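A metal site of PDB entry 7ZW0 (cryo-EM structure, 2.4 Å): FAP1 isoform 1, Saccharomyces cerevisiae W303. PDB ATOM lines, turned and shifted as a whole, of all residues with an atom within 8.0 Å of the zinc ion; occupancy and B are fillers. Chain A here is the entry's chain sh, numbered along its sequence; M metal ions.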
ATOM      1  N   LYS A 410     -14.743 -19.222  -4.393  1.00  0.00           N
ATOM      2  CA  LYS A 410     -15.192 -18.619  -5.634  1.00  0.00           C
ATOM      3  C   LYS A 410     -16.675 -18.314  -5.625  1.00  0.00           C
ATOM      4  O   LYS A 410     -17.451 -19.037  -5.004  1.00  0.00           O
ATOM      5  CB  LYS A 410     -14.830 -19.503  -6.832  1.00  0.00           C
ATOM      6  CG  LYS A 410     -13.797 -20.564  -6.504  1.00  0.00           C
ATOM      7  CD  LYS A 410     -12.806 -20.729  -7.652  1.00  0.00           C
ATOM      8  CE  LYS A 410     -11.924 -19.503  -7.782  1.00  0.00           C
ATOM      9  NZ  LYS A 410     -10.967 -19.615  -8.912  1.00  0.00           N
ATOM     10  N   CYS A 411     -17.057 -17.242  -6.290  1.00  0.00           N
ATOM     11  CA  CYS A 411     -18.462 -16.865  -6.379  1.00  0.00           C
ATOM     12  C   CYS A 411     -19.348 -18.001  -6.868  1.00  0.00           C
ATOM     13  O   CYS A 411     -20.409 -18.226  -6.308  1.00  0.00           O
ATOM     14  CB  CYS A 411     -18.602 -15.685  -7.349  1.00  0.00           C
ATOM     15  SG  CYS A 411     -20.288 -15.151  -7.677  1.00  0.00           S
ATOM     16  N   GLU A 412     -18.911 -18.709  -7.900  1.00  0.00           N
ATOM     17  CA  GLU A 412     -19.655 -19.873  -8.399  1.00  0.00           C
ATOM     18  C   GLU A 412     -21.122 -19.565  -8.711  1.00  0.00           C
ATOM     19  O   GLU A 412     -22.005 -20.360  -8.369  1.00  0.00           O
ATOM     20  CB  GLU A 412     -19.525 -21.053  -7.431  1.00  0.00           C
ATOM     21  CG  GLU A 412     -18.101 -21.509  -7.214  1.00  0.00           C
ATOM     22  CD  GLU A 412     -17.929 -22.316  -5.943  1.00  0.00           C
ATOM     23  OE1 GLU A 412     -16.788 -22.719  -5.642  1.00  0.00           O
ATOM     24  OE2 GLU A 412     -18.936 -22.534  -5.240  1.00  0.00           O
ATOM     25  N   SER A 413     -21.393 -18.415  -9.319  1.00  0.00           N
ATOM     26  CA  SER A 413     -22.774 -18.039  -9.620  1.00  0.00           C
ATOM     27  C   SER A 413     -22.981 -17.772 -11.099  1.00  0.00           C
ATOM     28  O   SER A 413     -22.035 -17.491 -11.823  1.00  0.00           O
ATOM     29  CB  SER A 413     -23.206 -16.827  -8.804  1.00  0.00           C
ATOM     30  OG  SER A 413     -23.080 -17.073  -7.416  1.00  0.00           O
ATOM     31  N   LEU A 414     -24.226 -17.841 -11.557  1.00  0.00           N
ATOM     32  CA  LEU A 414     -24.495 -17.683 -12.985  1.00  0.00           C
ATOM     33  C   LEU A 414     -24.189 -16.331 -13.591  1.00  0.00           C
ATOM     34  O   LEU A 414     -24.420 -15.290 -12.983  1.00  0.00           O
ATOM     35  CB  LEU A 414     -25.958 -18.033 -13.279  1.00  0.00           C
ATOM     36  CG  LEU A 414     -26.274 -19.530 -13.251  1.00  0.00           C
ATOM     37  CD1 LEU A 414     -27.753 -19.730 -13.550  1.00  0.00           C
ATOM     38  CD2 LEU A 414     -25.415 -20.259 -14.269  1.00  0.00           C
ATOM     39  N   MET A 415     -23.659 -16.341 -14.811  1.00  0.00           N
ATOM     40  CA  MET A 415     -23.405 -15.105 -15.538  1.00  0.00           C
ATOM     41  C   MET A 415     -24.711 -14.656 -16.181  1.00  0.00           C
ATOM     42  O   MET A 415     -25.708 -15.375 -16.106  1.00  0.00           O
ATOM     43  CB  MET A 415     -22.331 -15.311 -16.603  1.00  0.00           C
ATOM     44  CG  MET A 415     -21.019 -15.869 -16.067  1.00  0.00           C
ATOM     45  SD  MET A 415     -20.143 -14.789 -14.934  1.00  0.00           S
ATOM     46  CE  MET A 415     -19.188 -13.794 -16.075  1.00  0.00           C
ATOM     47  N   ARG A 421     -20.027 -19.877 -15.034  1.00  0.00           N
ATOM     48  CA  ARG A 421     -20.099 -19.538 -13.623  1.00  0.00           C
ATOM     49  C   ARG A 421     -19.013 -18.526 -13.249  1.00  0.00           C
ATOM     50  O   ARG A 421     -17.855 -18.703 -13.635  1.00  0.00           O
ATOM     51  CB  ARG A 421     -19.934 -20.789 -12.760  1.00  0.00           C
ATOM     52  CG  ARG A 421     -21.118 -21.752 -12.815  1.00  0.00           C
ATOM     53  CD  ARG A 421     -22.272 -21.247 -11.957  1.00  0.00           C
ATOM     54  NE  ARG A 421     -23.350 -22.228 -11.867  1.00  0.00           N
ATOM     55  CZ  ARG A 421     -24.411 -22.088 -11.081  1.00  0.00           C
ATOM     56  NH1 ARG A 421     -24.549 -21.010 -10.322  1.00  0.00           N
ATOM     57  NH2 ARG A 421     -25.343 -23.033 -11.050  1.00  0.00           N
ATOM     58  N   CYS A 422     -19.388 -17.478 -12.526  1.00  0.00           N
ATOM     59  CA  CYS A 422     -18.412 -16.497 -12.068  1.00  0.00           C
ATOM     60  C   CYS A 422     -17.344 -17.157 -11.206  1.00  0.00           C
ATOM     61  O   CYS A 422     -17.666 -17.924 -10.305  1.00  0.00           O
ATOM     62  CB  CYS A 422     -19.108 -15.395 -11.280  1.00  0.00           C
ATOM     63  SG  CYS A 422     -18.057 -13.995 -10.832  1.00  0.00           S
ATOM     64  N   THR A 423     -16.086 -16.863 -11.485  1.00  0.00           N
ATOM     65  CA  THR A 423     -14.993 -17.441 -10.696  1.00  0.00           C
ATOM     66  C   THR A 423     -14.389 -16.474  -9.692  1.00  0.00           C
ATOM     67  O   THR A 423     -13.448 -16.816  -8.982  1.00  0.00           O
ATOM     68  CB  THR A 423     -13.864 -17.964 -11.594  1.00  0.00           C
ATOM     69  OG1 THR A 423     -13.346 -16.878 -12.383  1.00  0.00           O
ATOM     70  CG2 THR A 423     -14.380 -19.056 -12.526  1.00  0.00           C
ATOM     71  N   ASP A 424     -14.919 -15.248  -9.629  1.00  0.00           N
ATOM     72  CA  ASP A 424     -14.333 -14.246  -8.745  1.00  0.00           C
ATOM     73  C   ASP A 424     -14.432 -14.613  -7.282  1.00  0.00           C
ATOM     74  O   ASP A 424     -15.484 -15.054  -6.820  1.00  0.00           O
ATOM     75  CB  ASP A 424     -14.985 -12.882  -8.986  1.00  0.00           C
ATOM     76  CG  ASP A 424     -14.767 -12.380 -10.397  1.00  0.00           C
ATOM     77  OD1 ASP A 424     -13.918 -12.953 -11.117  1.00  0.00           O
ATOM     78  OD2 ASP A 424     -15.446 -11.405 -10.798  1.00  0.00           O
ATOM     79  N   ARG A 425     -13.356 -14.403  -6.538  1.00  0.00           N
ATOM     80  CA  ARG A 425     -13.333 -14.724  -5.107  1.00  0.00           C
ATOM     81  C   ARG A 425     -14.054 -13.696  -4.252  1.00  0.00           C
ATOM     82  O   ARG A 425     -13.750 -12.507  -4.334  1.00  0.00           O
ATOM     83  CB  ARG A 425     -11.882 -14.825  -4.627  1.00  0.00           C
ATOM     84  CG  ARG A 425     -11.538 -16.120  -3.908  1.00  0.00           C
ATOM     85  CD  ARG A 425     -11.646 -17.295  -4.857  1.00  0.00           C
ATOM     86  NE  ARG A 425     -11.531 -18.577  -4.168  1.00  0.00           N
ATOM     87  CZ  ARG A 425     -10.397 -19.271  -4.062  1.00  0.00           C
ATOM     88  NH1 ARG A 425      -9.288 -18.804  -4.601  1.00  0.00           N
ATOM     89  NH2 ARG A 425     -10.383 -20.426  -3.411  1.00  0.00           N
ATOM     90  N   CYS A 426     -15.014 -14.145  -3.437  1.00  0.00           N
ATOM     91  CA  CYS A 426     -15.774 -13.237  -2.557  1.00  0.00           C
ATOM     92  C   CYS A 426     -16.362 -12.099  -3.380  1.00  0.00           C
ATOM     93  O   CYS A 426     -16.302 -10.939  -2.976  1.00  0.00           O
ATOM     94  CB  CYS A 426     -14.949 -12.728  -1.380  1.00  0.00           C
ATOM     95  SG  CYS A 426     -15.954 -12.359   0.079  1.00  0.00           S
ATOM     96  N   CYS A 427     -16.914 -12.433  -4.528  1.00  0.00           N
ATOM     97  CA  CYS A 427     -17.456 -11.439  -5.435  1.00  0.00           C
ATOM     98  C   CYS A 427     -18.516 -10.489  -4.862  1.00  0.00           C
ATOM     99  O   CYS A 427     -19.380 -10.919  -4.099  1.00  0.00           O
ATOM    100  CB  CYS A 427     -18.050 -12.231  -6.588  1.00  0.00           C
ATOM    101  SG  CYS A 427     -18.839 -11.297  -7.880  1.00  0.00           S
ATOM    102  N   SER A 428     -18.465  -9.207  -5.232  1.00  0.00           N
ATOM    103  CA  SER A 428     -19.481  -8.253  -4.783  1.00  0.00           C
ATOM    104  C   SER A 428     -20.845  -8.654  -5.317  1.00  0.00           C
ATOM    105  O   SER A 428     -21.852  -8.467  -4.663  1.00  0.00           O
ATOM    106  CB  SER A 428     -19.136  -6.834  -5.219  1.00  0.00           C
ATOM    107  OG  SER A 428     -19.186  -6.703  -6.620  1.00  0.00           O
ATOM    108  N   GLY A 429     -20.868  -9.164  -6.545  1.00  0.00           N
ATOM    109  CA  GLY A 429     -22.110  -9.606  -7.157  1.00  0.00           C
ATOM    110  C   GLY A 429     -22.823 -10.766  -6.491  1.00  0.00           C
ATOM    111  O   GLY A 429     -24.036 -10.876  -6.592  1.00  0.00           O
ATOM    112  N   ARG A 430     -22.079 -11.642  -5.813  1.00  0.00           N
ATOM    113  CA  ARG A 430     -22.698 -12.849  -5.250  1.00  0.00           C
ATOM    114  C   ARG A 430     -23.835 -12.690  -4.234  1.00  0.00           C
ATOM    115  O   ARG A 430     -24.833 -13.381  -4.335  1.00  0.00           O
ATOM    116  CB  ARG A 430     -21.607 -13.780  -4.671  1.00  0.00           C
ATOM    117  CG  ARG A 430     -22.154 -14.947  -3.873  1.00  0.00           C
ATOM    118  CD  ARG A 430     -21.161 -16.097  -3.776  1.00  0.00           C
ATOM    119  NE  ARG A 430     -21.677 -17.217  -2.998  1.00  0.00           N
ATOM    120  CZ  ARG A 430     -22.438 -18.189  -3.496  1.00  0.00           C
ATOM    121  NH1 ARG A 430     -22.767 -18.195  -4.779  1.00  0.00           N
ATOM    122  NH2 ARG A 430     -22.859 -19.169  -2.712  1.00  0.00           N
ATOM    123  N   PRO A 431     -23.718 -11.751  -3.279  1.00  0.00           N
ATOM    124  CA  PRO A 431     -24.863 -11.653  -2.357  1.00  0.00           C
ATOM    125  C   PRO A 431     -26.124 -11.266  -3.110  1.00  0.00           C
ATOM    126  O   PRO A 431     -27.200 -11.813  -2.835  1.00  0.00           O
ATOM    127  CB  PRO A 431     -24.452 -10.542  -1.391  1.00  0.00           C
ATOM    128  CG  PRO A 431     -23.319  -9.838  -2.048  1.00  0.00           C
ATOM    129  CD  PRO A 431     -22.606 -10.898  -2.815  1.00  0.00           C
ATOM    130  N   ALA A 433     -26.759 -11.898  -6.196  1.00  0.00           N
ATOM    131  CA  ALA A 433     -27.146 -13.056  -6.993  1.00  0.00           C
ATOM    132  C   ALA A 433     -27.934 -14.062  -6.166  1.00  0.00           C
ATOM    133  O   ALA A 433     -28.915 -14.627  -6.643  1.00  0.00           O
ATOM    134  CB  ALA A 433     -25.925 -13.725  -7.585  1.00  0.00           C
ATOM    135  N   GLU A 453     -26.716  -8.782 -11.905  1.00  0.00           N
ATOM    136  CA  GLU A 453     -25.742  -7.754 -11.534  1.00  0.00           C
ATOM    137  C   GLU A 453     -24.684  -7.511 -12.608  1.00  0.00           C
ATOM    138  O   GLU A 453     -24.305  -8.438 -13.323  1.00  0.00           O
ATOM    139  CB  GLU A 453     -25.096  -8.061 -10.178  1.00  0.00           C
ATOM    140  CG  GLU A 453     -24.646  -9.500  -9.996  1.00  0.00           C
ATOM    141  CD  GLU A 453     -25.776 -10.446  -9.635  1.00  0.00           C
ATOM    142  OE1 GLU A 453     -25.767 -11.585 -10.121  1.00  0.00           O
ATOM    143  OE2 GLU A 453     -26.692 -10.028  -8.892  1.00  0.00           O
ATOM    144  N   LYS A 455     -21.428  -7.000 -12.553  1.00  0.00           N
ATOM    145  CA  LYS A 455     -20.201  -7.760 -12.446  1.00  0.00           C
ATOM    146  C   LYS A 455     -20.413  -9.149 -13.024  1.00  0.00           C
ATOM    147  O   LYS A 455     -19.548  -9.668 -13.721  1.00  0.00           O
ATOM    148  CB  LYS A 455     -19.768  -7.857 -10.978  1.00  0.00           C
ATOM    149  CG  LYS A 455     -18.331  -8.317 -10.782  1.00  0.00           C
ATOM    150  CD  LYS A 455     -17.906  -8.140  -9.338  1.00  0.00           C
ATOM    151  CE  LYS A 455     -16.463  -8.559  -9.122  1.00  0.00           C
ATOM    152  NZ  LYS A 455     -16.084  -8.506  -7.677  1.00  0.00           N
ATOM    153  N   HIS A 456     -21.567  -9.736 -12.756  1.00  0.00           N
ATOM    154  CA  HIS A 456     -21.887 -11.059 -13.287  1.00  0.00           C
ATOM    155  C   HIS A 456     -22.129 -11.082 -14.800  1.00  0.00           C
ATOM    156  O   HIS A 456     -22.059 -12.139 -15.406  1.00  0.00           O
ATOM    157  CB  HIS A 456     -23.064 -11.690 -12.540  1.00  0.00           C
ATOM    158  CG  HIS A 456     -22.692 -12.198 -11.181  1.00  0.00           C
ATOM    159  ND1 HIS A 456     -23.341 -13.253 -10.588  1.00  0.00           N
ATOM    160  CD2 HIS A 456     -21.739 -11.795 -10.311  1.00  0.00           C
ATOM    161  CE1 HIS A 456     -22.812 -13.475  -9.391  1.00  0.00           C
ATOM    162  NE2 HIS A 456     -21.829 -12.610  -9.213  1.00  0.00           N
HETATM  163 ZN    ZN M   1     -19.660 -13.437  -8.597  1.00  0.00          ZN
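The backbone NH (N) of Cys 422 sits at hydrogen-bond distance from the backbone carbonyl oxygen (O) of Ser 413 (2.7 Å).
O of Cys 422 sits at hydrogen-bond distance from N of Glu 412, at 2.8 Å.
The backbone NH (N) of Cys 411 lies within hydrogen-bond range of the backbone carbonyl oxygen (O) of Asp 424 (2.7 Å).
The side-chain sulfur (SD) of Met 415 sits at hydrogen-bond distance from the backbone NH (N) of Cys 422.
O of Cys 411 sits at hydrogen-bond distance from OG of Ser 413 (3.1 Å).
ND1 of His 456 lies within hydrogen-bond range of O of Leu 414, 3.3 Å away.
The backbone NH of Gly 429 sits close to the side-chain sulfur of Cys 427 (3.2 Å).
NH1 of Arg 430 is in hydrogen-bond range of O of Cys 411 (2.8 Å).
The nearest printed residue that does not touch the zinc ion is Arg 430 (4.1 Å).
The zinc ion is bound by SG of Cys 411 (2.0 Å), SG of Cys 427 (2.4 Å) and NE2 of His 456 (2.4 Å).
Slightly farther from the zinc ion lies SG of Cys 422 (2.8 Å).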
